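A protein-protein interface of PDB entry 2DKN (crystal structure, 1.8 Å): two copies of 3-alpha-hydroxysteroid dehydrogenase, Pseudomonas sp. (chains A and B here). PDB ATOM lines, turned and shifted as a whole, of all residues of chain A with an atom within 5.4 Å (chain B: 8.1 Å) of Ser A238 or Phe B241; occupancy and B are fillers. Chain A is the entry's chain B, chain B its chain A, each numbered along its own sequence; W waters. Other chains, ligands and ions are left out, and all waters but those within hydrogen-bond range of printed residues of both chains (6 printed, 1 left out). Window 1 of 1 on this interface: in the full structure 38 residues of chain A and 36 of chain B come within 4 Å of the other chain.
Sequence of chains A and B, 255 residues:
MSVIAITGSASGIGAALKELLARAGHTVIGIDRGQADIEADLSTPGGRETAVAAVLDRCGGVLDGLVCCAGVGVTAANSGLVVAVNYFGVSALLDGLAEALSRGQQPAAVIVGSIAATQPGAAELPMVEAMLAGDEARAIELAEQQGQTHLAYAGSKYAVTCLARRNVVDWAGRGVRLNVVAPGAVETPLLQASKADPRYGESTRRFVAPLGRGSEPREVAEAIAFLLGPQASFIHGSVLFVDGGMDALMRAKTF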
ATOM      1  N   ARG A 165     -14.467  -9.808   6.537  1.00  0.00           N
ATOM      2  CA  ARG A 165     -14.924 -10.757   7.546  1.00  0.00           C
ATOM      3  C   ARG A 165     -15.980 -10.149   8.469  1.00  0.00           C
ATOM      4  O   ARG A 165     -16.930 -10.814   8.892  1.00  0.00           O
ATOM      5  CB  ARG A 165     -13.731 -11.266   8.354  1.00  0.00           C
ATOM      6  CG  ARG A 165     -12.794 -12.142   7.497  1.00  0.00           C
ATOM      7  CD  ARG A 165     -11.462 -12.436   8.183  1.00  0.00           C
ATOM      8  NE  ARG A 165     -11.547 -13.355   9.336  1.00  0.00           N
ATOM      9  CZ  ARG A 165     -11.713 -14.682   9.235  1.00  0.00           C
ATOM     10  NH1 ARG A 165     -11.864 -15.256   8.049  1.00  0.00           N
ATOM     11  NH2 ARG A 165     -11.719 -15.446  10.329  1.00  0.00           N
ATOM     12  N   LEU A 178     -18.916 -13.415   0.183  1.00  0.00           N
ATOM     13  CA  LEU A 178     -17.795 -12.485   0.083  1.00  0.00           C
ATOM     14  C   LEU A 178     -16.539 -13.139   0.674  1.00  0.00           C
ATOM     15  O   LEU A 178     -16.540 -13.523   1.839  1.00  0.00           O
ATOM     16  CB  LEU A 178     -18.106 -11.217   0.870  1.00  0.00           C
ATOM     17  CG  LEU A 178     -16.989 -10.173   0.936  1.00  0.00           C
ATOM     18  CD1 LEU A 178     -16.584  -9.753  -0.481  1.00  0.00           C
ATOM     19  CD2 LEU A 178     -17.421  -8.948   1.809  1.00  0.00           C
ATOM     20  N   ASN A 179     -15.477 -13.255  -0.116  1.00  0.00           N
ATOM     21  CA  ASN A 179     -14.244 -13.891   0.342  1.00  0.00           C
ATOM     22  C   ASN A 179     -13.045 -13.002  -0.036  1.00  0.00           C
ATOM     23  O   ASN A 179     -13.197 -12.077  -0.868  1.00  0.00           O
ATOM     24  CB  ASN A 179     -14.110 -15.286  -0.300  1.00  0.00           C
ATOM     25  CG  ASN A 179     -15.147 -16.256   0.221  1.00  0.00           C
ATOM     26  OD1 ASN A 179     -15.082 -16.664   1.392  1.00  0.00           O
ATOM     27  ND2 ASN A 179     -16.146 -16.584  -0.607  1.00  0.00           N
ATOM     28  N   VAL A 180     -11.874 -13.286   0.550  1.00  0.00           N
ATOM     29  CA  VAL A 180     -10.641 -12.586   0.224  1.00  0.00           C
ATOM     30  C   VAL A 180      -9.603 -13.563  -0.343  1.00  0.00           C
ATOM     31  O   VAL A 180      -9.466 -14.691   0.153  1.00  0.00           O
ATOM     32  CB  VAL A 180     -10.063 -11.924   1.493  1.00  0.00           C
ATOM     33  CG1 VAL A 180      -8.753 -11.190   1.165  1.00  0.00           C
ATOM     34  CG2 VAL A 180     -11.106 -11.007   2.104  1.00  0.00           C
ATOM     35  N   PHE A 234     -20.300 -22.999  -0.409  1.00  0.00           N
ATOM     36  CA  PHE A 234     -20.319 -22.911   1.059  1.00  0.00           C
ATOM     37  C   PHE A 234     -19.131 -22.158   1.645  1.00  0.00           C
ATOM     38  O   PHE A 234     -18.875 -22.208   2.848  1.00  0.00           O
ATOM     39  CB  PHE A 234     -20.502 -24.277   1.723  1.00  0.00           C
ATOM     40  CG  PHE A 234     -21.143 -24.195   3.091  1.00  0.00           C
ATOM     41  CD1 PHE A 234     -20.444 -24.571   4.223  1.00  0.00           C
ATOM     42  CD2 PHE A 234     -22.442 -23.695   3.232  1.00  0.00           C
ATOM     43  CE1 PHE A 234     -21.051 -24.496   5.506  1.00  0.00           C
ATOM     44  CE2 PHE A 234     -23.036 -23.605   4.490  1.00  0.00           C
ATOM     45  CZ  PHE A 234     -22.337 -24.017   5.617  1.00  0.00           C
ATOM     46  N   ILE A 235     -18.420 -21.421   0.794  1.00  0.00           N
ATOM     47  CA  ILE A 235     -17.236 -20.709   1.252  1.00  0.00           C
ATOM     48  C   ILE A 235     -17.598 -19.233   1.376  1.00  0.00           C
ATOM     49  O   ILE A 235     -17.952 -18.591   0.384  1.00  0.00           O
ATOM     50  CB  ILE A 235     -16.021 -20.912   0.289  1.00  0.00           C
ATOM     51  CG1 ILE A 235     -15.685 -22.412   0.133  1.00  0.00           C
ATOM     52  CG2 ILE A 235     -14.819 -20.153   0.822  1.00  0.00           C
ATOM     53  CD1 ILE A 235     -14.685 -22.712  -0.977  1.00  0.00           C
ATOM     54  N   HIS A 236     -17.518 -18.699   2.591  1.00  0.00           N
ATOM     55  CA  HIS A 236     -17.961 -17.341   2.832  1.00  0.00           C
ATOM     56  C   HIS A 236     -17.166 -16.779   3.990  1.00  0.00           C
ATOM     57  O   HIS A 236     -17.003 -17.433   5.027  1.00  0.00           O
ATOM     58  CB  HIS A 236     -19.470 -17.360   3.150  1.00  0.00           C
ATOM     59  CG  HIS A 236     -20.053 -16.013   3.453  1.00  0.00           C
ATOM     60  ND1 HIS A 236     -19.822 -14.908   2.663  1.00  0.00           N
ATOM     61  CD2 HIS A 236     -20.900 -15.607   4.434  1.00  0.00           C
ATOM     62  CE1 HIS A 236     -20.470 -13.867   3.162  1.00  0.00           C
ATOM     63  NE2 HIS A 236     -21.148 -14.269   4.229  1.00  0.00           N
ATOM     64  N   GLY A 237     -16.637 -15.576   3.796  1.00  0.00           N
ATOM     65  CA  GLY A 237     -15.795 -14.947   4.810  1.00  0.00           C
ATOM     66  C   GLY A 237     -14.397 -15.531   4.922  1.00  0.00           C
ATOM     67  O   GLY A 237     -13.635 -15.144   5.807  1.00  0.00           O
ATOM     68  N   SER A 238     -14.015 -16.422   3.999  1.00  0.00           N
ATOM     69  CA  SER A 238     -12.693 -17.021   4.068  1.00  0.00           C
ATOM     70  C   SER A 238     -11.627 -16.121   3.468  1.00  0.00           C
ATOM     71  O   SER A 238     -11.885 -15.406   2.512  1.00  0.00           O
ATOM     72  CB  SER A 238     -12.656 -18.368   3.301  1.00  0.00           C
ATOM     73  OG  SER A 238     -13.372 -19.349   4.017  1.00  0.00           O
ATOM     74  N   VAL A 239     -10.399 -16.277   3.979  1.00  0.00           N
ATOM     75  CA  VAL A 239      -9.214 -15.657   3.403  1.00  0.00           C
ATOM     76  C   VAL A 239      -8.362 -16.796   2.808  1.00  0.00           C
ATOM     77  O   VAL A 239      -7.788 -17.621   3.537  1.00  0.00           O
ATOM     78  CB  VAL A 239      -8.416 -14.850   4.438  1.00  0.00           C
ATOM     79  CG1 VAL A 239      -7.189 -14.199   3.787  1.00  0.00           C
ATOM     80  CG2 VAL A 239      -9.315 -13.790   5.089  1.00  0.00           C
ATOM     81  N   LEU A 240      -8.311 -16.853   1.482  1.00  0.00           N
ATOM     82  CA  LEU A 240      -7.543 -17.889   0.811  1.00  0.00           C
ATOM     83  C   LEU A 240      -6.171 -17.354   0.445  1.00  0.00           C
ATOM     84  O   LEU A 240      -6.049 -16.531  -0.454  1.00  0.00           O
ATOM     85  CB  LEU A 240      -8.271 -18.309  -0.461  1.00  0.00           C
ATOM     86  CG  LEU A 240      -7.575 -19.400  -1.300  1.00  0.00           C
ATOM     87  CD1 LEU A 240      -7.203 -20.606  -0.422  1.00  0.00           C
ATOM     88  CD2 LEU A 240      -8.524 -19.805  -2.406  1.00  0.00           C
ATOM     89  N   PHE A 255      -3.721 -19.625  12.172  1.00  0.00           N
ATOM     90  CA  PHE A 255      -4.773 -19.917  11.224  1.00  0.00           C
ATOM     91  C   PHE A 255      -6.073 -19.856  12.003  1.00  0.00           C
ATOM     92  O   PHE A 255      -6.080 -19.821  13.255  1.00  0.00           O
ATOM     93  CB  PHE A 255      -4.550 -21.276  10.539  1.00  0.00           C
ATOM     94  CG  PHE A 255      -4.423 -22.414  11.490  1.00  0.00           C
ATOM     95  CD1 PHE A 255      -5.554 -23.079  11.949  1.00  0.00           C
ATOM     96  CD2 PHE A 255      -3.173 -22.811  11.948  1.00  0.00           C
ATOM     97  CE1 PHE A 255      -5.430 -24.131  12.852  1.00  0.00           C
ATOM     98  CE2 PHE A 255      -3.043 -23.851  12.844  1.00  0.00           C
ATOM     99  CZ  PHE A 255      -4.175 -24.511  13.297  1.00  0.00           C
ATOM    100  OXT PHE A 255      -7.145 -19.802  11.419  1.00  0.00           O
ATOM    101  N   SER B 114     -10.889 -29.149  10.479  1.00  0.00           N
ATOM    102  CA  SER B 114     -12.137 -28.763  11.141  1.00  0.00           C
ATOM    103  C   SER B 114     -12.018 -27.375  11.727  1.00  0.00           C
ATOM    104  O   SER B 114     -10.943 -26.974  12.193  1.00  0.00           O
ATOM    105  CB  SER B 114     -12.463 -29.738  12.284  1.00  0.00           C
ATOM    106  OG  SER B 114     -13.672 -29.343  12.927  1.00  0.00           O
ATOM    107  N   ILE B 115     -13.133 -26.642  11.724  1.00  0.00           N
ATOM    108  CA  ILE B 115     -13.218 -25.377  12.410  1.00  0.00           C
ATOM    109  C   ILE B 115     -12.964 -25.605  13.913  1.00  0.00           C
ATOM    110  O   ILE B 115     -12.572 -24.681  14.615  1.00  0.00           O
ATOM    111  CB  ILE B 115     -14.615 -24.717  12.141  1.00  0.00           C
ATOM    112  CG1 ILE B 115     -14.697 -23.292  12.654  1.00  0.00           C
ATOM    113  CG2 ILE B 115     -15.717 -25.539  12.701  1.00  0.00           C
ATOM    114  CD1 ILE B 115     -15.930 -22.571  12.111  1.00  0.00           C
ATOM    115  N   ALA B 116     -13.135 -26.846  14.383  1.00  0.00           N
ATOM    116  CA  ALA B 116     -12.849 -27.173  15.788  1.00  0.00           C
ATOM    117  C   ALA B 116     -11.397 -26.884  16.122  1.00  0.00           C
ATOM    118  O   ALA B 116     -11.064 -26.640  17.272  1.00  0.00           O
ATOM    119  CB  ALA B 116     -13.195 -28.635  16.105  1.00  0.00           C
ATOM    120  N   ALA B 117     -10.528 -26.883  15.107  1.00  0.00           N
ATOM    121  CA  ALA B 117      -9.125 -26.534  15.316  1.00  0.00           C
ATOM    122  C   ALA B 117      -8.934 -25.151  15.953  1.00  0.00           C
ATOM    123  O   ALA B 117      -7.885 -24.879  16.534  1.00  0.00           O
ATOM    124  CB  ALA B 117      -8.369 -26.604  14.021  1.00  0.00           C
ATOM    125  N   THR B 118      -9.926 -24.278  15.798  1.00  0.00           N
ATOM    126  CA  THR B 118      -9.801 -22.889  16.223  1.00  0.00           C
ATOM    127  C   THR B 118     -10.397 -22.665  17.613  1.00  0.00           C
ATOM    128  O   THR B 118     -10.435 -21.525  18.100  1.00  0.00           O
ATOM    129  CB  THR B 118     -10.528 -21.951  15.243  1.00  0.00           C
ATOM    130  OG1 THR B 118     -11.934 -22.219  15.279  1.00  0.00           O
ATOM    131  CG2 THR B 118     -10.033 -22.185  13.817  1.00  0.00           C
ATOM    132  N   THR B 161      -3.621 -29.766  11.528  1.00  0.00           N
ATOM    133  CA  THR B 161      -3.543 -28.533  10.709  1.00  0.00           C
ATOM    134  C   THR B 161      -2.158 -27.895  10.798  1.00  0.00           C
ATOM    135  O   THR B 161      -1.562 -27.536   9.767  1.00  0.00           O
ATOM    136  CB  THR B 161      -4.709 -27.547  11.060  1.00  0.00           C
ATOM    137  OG1 THR B 161      -5.958 -28.236  10.893  1.00  0.00           O
ATOM    138  CG2 THR B 161      -4.710 -26.325  10.135  1.00  0.00           C
ATOM    139  N   VAL B 180      -5.007 -27.765   3.689  1.00  0.00           N
ATOM    140  CA  VAL B 180      -6.044 -28.261   4.603  1.00  0.00           C
ATOM    141  C   VAL B 180      -7.372 -27.607   4.266  1.00  0.00           C
ATOM    142  O   VAL B 180      -7.412 -26.410   3.984  1.00  0.00           O
ATOM    143  CB  VAL B 180      -5.697 -27.878   6.053  1.00  0.00           C
ATOM    144  CG1 VAL B 180      -6.788 -28.363   7.038  1.00  0.00           C
ATOM    145  CG2 VAL B 180      -4.312 -28.415   6.443  1.00  0.00           C
ATOM    146  N   VAL B 181      -8.445 -28.399   4.259  1.00  0.00           N
ATOM    147  CA  VAL B 181      -9.800 -27.854   4.186  1.00  0.00           C
ATOM    148  C   VAL B 181     -10.390 -27.962   5.579  1.00  0.00           C
ATOM    149  O   VAL B 181     -10.288 -29.005   6.222  1.00  0.00           O
ATOM    150  CB  VAL B 181     -10.646 -28.601   3.116  1.00  0.00           C
ATOM    151  CG1 VAL B 181     -12.090 -28.272   3.242  1.00  0.00           C
ATOM    152  CG2 VAL B 181     -10.145 -28.202   1.708  1.00  0.00           C
ATOM    153  N   ALA B 182     -10.981 -26.874   6.049  1.00  0.00           N
ATOM    154  CA  ALA B 182     -11.545 -26.830   7.391  1.00  0.00           C
ATOM    155  C   ALA B 182     -13.055 -26.598   7.328  1.00  0.00           C
ATOM    156  O   ALA B 182     -13.534 -25.449   7.250  1.00  0.00           O
ATOM    157  CB  ALA B 182     -10.846 -25.755   8.233  1.00  0.00           C
ATOM    158  N   PRO B 183     -13.819 -27.695   7.328  1.00  0.00           N
ATOM    159  CA  PRO B 183     -15.277 -27.566   7.273  1.00  0.00           C
ATOM    160  C   PRO B 183     -15.852 -27.069   8.597  1.00  0.00           C
ATOM    161  O   PRO B 183     -15.256 -27.279   9.657  1.00  0.00           O
ATOM    162  CB  PRO B 183     -15.765 -29.008   7.004  1.00  0.00           C
ATOM    163  CG  PRO B 183     -14.538 -29.794   6.617  1.00  0.00           C
ATOM    164  CD  PRO B 183     -13.373 -29.100   7.307  1.00  0.00           C
ATOM    165  N   GLY B 184     -16.989 -26.379   8.510  1.00  0.00           N
ATOM    166  CA  GLY B 184     -17.826 -26.125   9.663  1.00  0.00           C
ATOM    167  C   GLY B 184     -18.804 -27.288   9.581  1.00  0.00           C
ATOM    168  O   GLY B 184     -18.445 -28.368   9.103  1.00  0.00           O
ATOM    169  N   VAL B 220     -18.116 -29.464   0.317  1.00  0.00           N
ATOM    170  CA  VAL B 220     -16.758 -29.657   0.828  1.00  0.00           C
ATOM    171  C   VAL B 220     -15.903 -30.397  -0.193  1.00  0.00           C
ATOM    172  O   VAL B 220     -14.756 -30.025  -0.422  1.00  0.00           O
ATOM    173  CB  VAL B 220     -16.744 -30.372   2.188  1.00  0.00           C
ATOM    174  CG1 VAL B 220     -15.284 -30.635   2.637  1.00  0.00           C
ATOM    175  CG2 VAL B 220     -17.479 -29.508   3.226  1.00  0.00           C
ATOM    176  N   ALA B 223     -14.463 -28.049  -2.830  1.00  0.00           N
ATOM    177  CA  ALA B 223     -13.275 -27.325  -2.339  1.00  0.00           C
ATOM    178  C   ALA B 223     -12.021 -28.214  -2.330  1.00  0.00           C
ATOM    179  O   ALA B 223     -10.915 -27.782  -2.713  1.00  0.00           O
ATOM    180  CB  ALA B 223     -13.545 -26.765  -0.976  1.00  0.00           C
ATOM    181  N   LEU B 227      -8.478 -27.791  -4.643  1.00  0.00           N
ATOM    182  CA  LEU B 227      -7.126 -27.745  -4.080  1.00  0.00           C
ATOM    183  C   LEU B 227      -6.246 -28.859  -4.619  1.00  0.00           C
ATOM    184  O   LEU B 227      -5.026 -28.712  -4.675  1.00  0.00           O
ATOM    185  CB  LEU B 227      -7.158 -27.759  -2.547  1.00  0.00           C
ATOM    186  CG  LEU B 227      -7.792 -26.505  -1.907  1.00  0.00           C
ATOM    187  CD1 LEU B 227      -7.963 -26.750  -0.424  1.00  0.00           C
ATOM    188  CD2 LEU B 227      -6.900 -25.285  -2.140  1.00  0.00           C
ATOM    189  N   SER B 238      -1.936 -23.754   2.735  1.00  0.00           N
ATOM    190  CA  SER B 238      -3.091 -22.932   3.095  1.00  0.00           C
ATOM    191  C   SER B 238      -4.148 -23.739   3.831  1.00  0.00           C
ATOM    192  O   SER B 238      -4.281 -24.959   3.648  1.00  0.00           O
ATOM    193  CB  SER B 238      -3.754 -22.293   1.867  1.00  0.00           C
ATOM    194  OG  SER B 238      -2.946 -21.289   1.278  1.00  0.00           O
ATOM    195  N   VAL B 239      -4.914 -23.029   4.661  1.00  0.00           N
ATOM    196  CA  VAL B 239      -6.081 -23.617   5.312  1.00  0.00           C
ATOM    197  C   VAL B 239      -7.318 -22.942   4.714  1.00  0.00           C
ATOM    198  O   VAL B 239      -7.537 -21.733   4.896  1.00  0.00           O
ATOM    199  CB  VAL B 239      -6.076 -23.383   6.837  1.00  0.00           C
ATOM    200  CG1 VAL B 239      -7.293 -24.069   7.468  1.00  0.00           C
ATOM    201  CG2 VAL B 239      -4.780 -23.898   7.459  1.00  0.00           C
ATOM    202  N   LEU B 240      -8.122 -23.722   4.001  1.00  0.00           N
ATOM    203  CA  LEU B 240      -9.306 -23.148   3.346  1.00  0.00           C
ATOM    204  C   LEU B 240     -10.517 -23.478   4.189  1.00  0.00           C
ATOM    205  O   LEU B 240     -10.903 -24.645   4.274  1.00  0.00           O
ATOM    206  CB  LEU B 240      -9.466 -23.785   1.972  1.00  0.00           C
ATOM    207  CG  LEU B 240     -10.157 -23.029   0.828  1.00  0.00           C
ATOM    208  CD1 LEU B 240     -10.771 -23.926  -0.252  1.00  0.00           C
ATOM    209  CD2 LEU B 240     -11.059 -21.863   1.211  1.00  0.00           C
ATOM    210  N   PHE B 241     -11.102 -22.474   4.838  1.00  0.00           N
ATOM    211  CA  PHE B 241     -12.332 -22.711   5.617  1.00  0.00           C
ATOM    212  C   PHE B 241     -13.510 -22.849   4.645  1.00  0.00           C
ATOM    213  O   PHE B 241     -13.609 -22.095   3.677  1.00  0.00           O
ATOM    214  CB  PHE B 241     -12.571 -21.578   6.609  1.00  0.00           C
ATOM    215  CG  PHE B 241     -11.699 -21.650   7.837  1.00  0.00           C
ATOM    216  CD1 PHE B 241     -12.223 -22.131   9.042  1.00  0.00           C
ATOM    217  CD2 PHE B 241     -10.370 -21.252   7.790  1.00  0.00           C
ATOM    218  CE1 PHE B 241     -11.430 -22.202  10.203  1.00  0.00           C
ATOM    219  CE2 PHE B 241      -9.547 -21.326   8.944  1.00  0.00           C
ATOM    220  CZ  PHE B 241     -10.102 -21.800  10.154  1.00  0.00           C
ATOM    221  N   VAL B 242     -14.367 -23.846   4.894  1.00  0.00           N
ATOM    222  CA  VAL B 242     -15.536 -24.137   4.055  1.00  0.00           C
ATOM    223  C   VAL B 242     -16.674 -24.306   5.049  1.00  0.00           C
ATOM    224  O   VAL B 242     -17.074 -25.426   5.398  1.00  0.00           O
ATOM    225  CB  VAL B 242     -15.331 -25.398   3.204  1.00  0.00           C
ATOM    226  CG1 VAL B 242     -16.577 -25.685   2.361  1.00  0.00           C
ATOM    227  CG2 VAL B 242     -14.118 -25.215   2.307  1.00  0.00           C
ATOM    228  N   ASP B 243     -17.086 -23.159   5.577  1.00  0.00           N
ATOM    229  CA  ASP B 243     -17.930 -23.146   6.769  1.00  0.00           C
ATOM    230  C   ASP B 243     -19.105 -22.154   6.756  1.00  0.00           C
ATOM    231  O   ASP B 243     -19.687 -21.858   7.800  1.00  0.00           O
ATOM    232  CB  ASP B 243     -17.008 -22.850   7.958  1.00  0.00           C
ATOM    233  CG  ASP B 243     -16.491 -21.404   7.970  1.00  0.00           C
ATOM    234  OD1 ASP B 243     -16.781 -20.601   7.050  1.00  0.00           O
ATOM    235  OD2 ASP B 243     -15.765 -21.085   8.905  1.00  0.00           O
ATOM    236  N   GLY B 244     -19.466 -21.654   5.583  1.00  0.00           N
ATOM    237  CA  GLY B 244     -20.629 -20.770   5.503  1.00  0.00           C
ATOM    238  C   GLY B 244     -20.506 -19.483   6.308  1.00  0.00           C
ATOM    239  O   GLY B 244     -21.521 -18.846   6.610  1.00  0.00           O
ATOM    240  N   GLY B 245     -19.276 -19.074   6.625  1.00  0.00           N
ATOM    241  CA  GLY B 245     -19.032 -17.822   7.347  1.00  0.00           C
ATOM    242  C   GLY B 245     -18.795 -17.955   8.847  1.00  0.00           C
ATOM    243  O   GLY B 245     -18.573 -16.956   9.531  1.00  0.00           O
ATOM    244  N   MET B 246     -18.816 -19.180   9.357  1.00  0.00           N
ATOM    245  CA  MET B 246     -18.743 -19.367  10.832  1.00  0.00           C
ATOM    246  C   MET B 246     -17.453 -18.837  11.425  1.00  0.00           C
ATOM    247  O   MET B 246     -17.469 -18.124  12.430  1.00  0.00           O
ATOM    248  CB  MET B 246     -18.955 -20.836  11.232  1.00  0.00           C
ATOM    249  CG  MET B 246     -19.139 -21.004  12.769  1.00  0.00           C
ATOM    250  SD  MET B 246     -20.593 -20.037  13.309  1.00  0.00           S
ATOM    251  CE  MET B 246     -21.667 -21.316  13.901  1.00  0.00           C
ATOM    252  N   ASP B 247     -16.306 -19.171  10.824  1.00  0.00           N
ATOM    253  CA  ASP B 247     -15.047 -18.686  11.380  1.00  0.00           C
ATOM    254  C   ASP B 247     -14.883 -17.163  11.253  1.00  0.00           C
ATOM    255  O   ASP B 247     -14.365 -16.508  12.148  1.00  0.00           O
ATOM    256  CB  ASP B 247     -13.864 -19.376  10.686  1.00  0.00           C
ATOM    257  CG  ASP B 247     -12.545 -18.903  11.207  1.00  0.00           C
ATOM    258  OD1 ASP B 247     -12.268 -19.176  12.398  1.00  0.00           O
ATOM    259  OD2 ASP B 247     -11.786 -18.295  10.421  1.00  0.00           O
ATOM    260  N   ALA B 248     -15.312 -16.595  10.133  1.00  0.00           N
ATOM    261  CA  ALA B 248     -15.270 -15.151   9.994  1.00  0.00           C
ATOM    262  C   ALA B 248     -16.155 -14.490  11.049  1.00  0.00           C
ATOM    263  O   ALA B 248     -15.825 -13.401  11.535  1.00  0.00           O
ATOM    264  CB  ALA B 248     -15.718 -14.745   8.602  1.00  0.00           C
ATOM    265  N   ARG B 251     -14.186 -15.276  14.649  1.00  0.00           N
ATOM    266  CA  ARG B 251     -12.809 -14.795  14.783  1.00  0.00           C
ATOM    267  C   ARG B 251     -12.519 -13.818  13.648  1.00  0.00           C
ATOM    268  O   ARG B 251     -11.668 -14.090  12.804  1.00  0.00           O
ATOM    269  CB  ARG B 251     -11.800 -15.952  14.702  1.00  0.00           C
ATOM    270  CG  ARG B 251     -11.992 -17.108  15.698  1.00  0.00           C
ATOM    271  CD  ARG B 251     -10.773 -18.079  15.656  1.00  0.00           C
ATOM    272  NE  ARG B 251     -10.455 -18.464  14.277  1.00  0.00           N
ATOM    273  CZ  ARG B 251      -9.258 -18.852  13.859  1.00  0.00           C
ATOM    274  NH1 ARG B 251      -8.249 -18.932  14.720  1.00  0.00           N
ATOM    275  NH2 ARG B 251      -9.066 -19.169  12.579  1.00  0.00           N
ATOM    276  N   THR B 254      -8.787 -12.714  12.787  1.00  0.00           N
ATOM    277  CA  THR B 254      -7.752 -13.739  12.728  1.00  0.00           C
ATOM    278  C   THR B 254      -7.539 -14.304  11.337  1.00  0.00           C
ATOM    279  O   THR B 254      -8.436 -14.904  10.747  1.00  0.00           O
ATOM    280  CB  THR B 254      -8.049 -14.885  13.709  1.00  0.00           C
ATOM    281  OG1 THR B 254      -8.146 -14.336  15.027  1.00  0.00           O
ATOM    282  CG2 THR B 254      -6.919 -15.898  13.686  1.00  0.00           C
ATOM    283  N   PHE B 255      -6.334 -14.115  10.821  1.00  0.00           N
ATOM    284  CA  PHE B 255      -5.930 -14.651   9.523  1.00  0.00           C
ATOM    285  C   PHE B 255      -4.440 -14.402   9.405  1.00  0.00           C
ATOM    286  O   PHE B 255      -3.860 -13.681  10.227  1.00  0.00           O
ATOM    287  CB  PHE B 255      -6.687 -13.973   8.364  1.00  0.00           C
ATOM    288  CG  PHE B 255      -6.672 -12.473   8.433  1.00  0.00           C
ATOM    289  CD1 PHE B 255      -7.726 -11.786   9.008  1.00  0.00           C
ATOM    290  CD2 PHE B 255      -5.592 -11.756   7.947  1.00  0.00           C
ATOM    291  CE1 PHE B 255      -7.712 -10.396   9.089  1.00  0.00           C
ATOM    292  CE2 PHE B 255      -5.571 -10.339   8.040  1.00  0.00           C
ATOM    293  CZ  PHE B 255      -6.631  -9.686   8.614  1.00  0.00           C
ATOM    294  OXT PHE B 255      -3.766 -14.890   8.505  1.00  0.00           O
HETATM  295  O   HOH W   1     -17.460 -11.117  11.593  1.00  0.00           O
HETATM  296  O   HOH W   2     -16.063 -20.472   4.413  1.00  0.00           O
HETATM  297  O   HOH W   3      -6.022 -19.630   3.191  1.00  0.00           O
HETATM  298  O   HOH W   4      -9.609 -19.989   4.438  1.00  0.00           O
HETATM  299  O   HOH W   5     -12.508 -18.099   7.799  1.00  0.00           O
HETATM  300  O   HOH W   6     -15.455 -18.209   7.461  1.00  0.00           O
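The side-chain hydroxyl of Ser A238 lies within hydrogen-bond range of the backbone carbonyl oxygen of Phe B241 (2.8 Å).
NH2 of Arg A165 sits at hydrogen-bond distance from O of Thr B254, at 3.4 Å.
N of Gly B245 sits close to O of His A236 (3.2 Å).
The side-chain carboxylate (OD2) of Asp B247 is in salt-bridge range of the guanidinium group (NH2) of Arg A165 (2.9 Å).
O of Phe A234 lies within hydrogen-bond range of N of Asp B243 (3.4 Å).
O of Arg B251 is in hydrogen-bond range of NH2 of Arg A165, at 2.8 Å.
O of Phe A234 is in hydrogen-bond range of N of Gly B244, 2.9 Å away.
O of Phe A255 lies within salt-bridge range of NH1 of Arg B251, at 2.8 Å.
Water W4 lies within hydrogen-bond range of O of Val B239, N of Phe B241 and O of Val A239.
Water W6 lies within hydrogen-bond range of OD1 of Asp B243 (2.8 Å), O of His A236 (3.0 Å) and N of Ala B248 (3.1 Å).
Water W1 lies within hydrogen-bond range of the backbone carbonyl oxygen of Arg A165 (2.8 Å) and the backbone carbonyl oxygen of Ala B248 (2.8 Å).
Positions printed for both chains: 180, 238, 239, 240 and 255.
Of the 18 pairs that touch across the chains among the printed residues, none has its exchanged pair printed and touching as well.
Gly A237 touches just one residue of chain B: Ala B248 (3.5 Å).
Ser A238 touches just one residue of chain B: Phe B241.
Ser B114 touches none of the printed residues of chain A.
Of chain A, only Ile A235 (3.7 Å), Ser A238 (2.8 Å) and Phe A255 (3.8 Å) come within 4 Å of Phe B241.
Of the printed residues of chain A, Gly B244 touches Phe A234 (2.9 Å) and His A236 (3.9 Å).
Printed residues of chain A within 4 Å of Asp B247: Arg A165 (2.9 Å).
The nearest residue of chain B that does not touch Ser A238 is Leu B240 (4.4 Å).
The nearest residue of chain A that does not touch Phe B241 is His A236 (5.3 Å).
The backbone NH of His A236 lies close to the side-chain amide oxygen of Asn A179 (3.4 Å).
OD2 of Asp B243 is in hydrogen-bond range of N of Asp B247.
The backbone carbonyl oxygen (O) of Ser A238 lies within hydrogen-bond range of the backbone NH (N) of Val A180.
The backbone NH of Met B246 sits at hydrogen-bond distance from the side-chain carboxylate of Asp B243.
Among the printed residues, pairs that only touch across the chains: Gly A237 with Ala B248, Phe A255 with Thr B161, Arg A165 with Ala B248, Ile A235 with Phe B241, Phe A234 with Val B242, His A236 with Asp B243, Phe A255 with Phe B241, Ile A235 with Val B242, Arg A165 with Phe B255 and His A236 with Gly B244.
Hydrophobic or aromatic side chains of chain A that line the printed part of chain B: Phe A234, Ile A235, His A236 and Phe A255.
Of the 28 printed residues of chain B, 11 touch a printed residue of chain A.
Hydrophobic or aromatic side chains of chain B within 4 Å of the printed part of chain A: Phe B241, Val B242, Ala B248 and Phe B255.
Along chain B the printed residues that touch a printed residue of chain A span positions 161 to 255.
Among the printed residues, Asp or Glu carboxylates within 4 Å of a Lys or Arg side-chain nitrogen of the other chain: Arg A165 with Asp B247 (2.9 Å).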
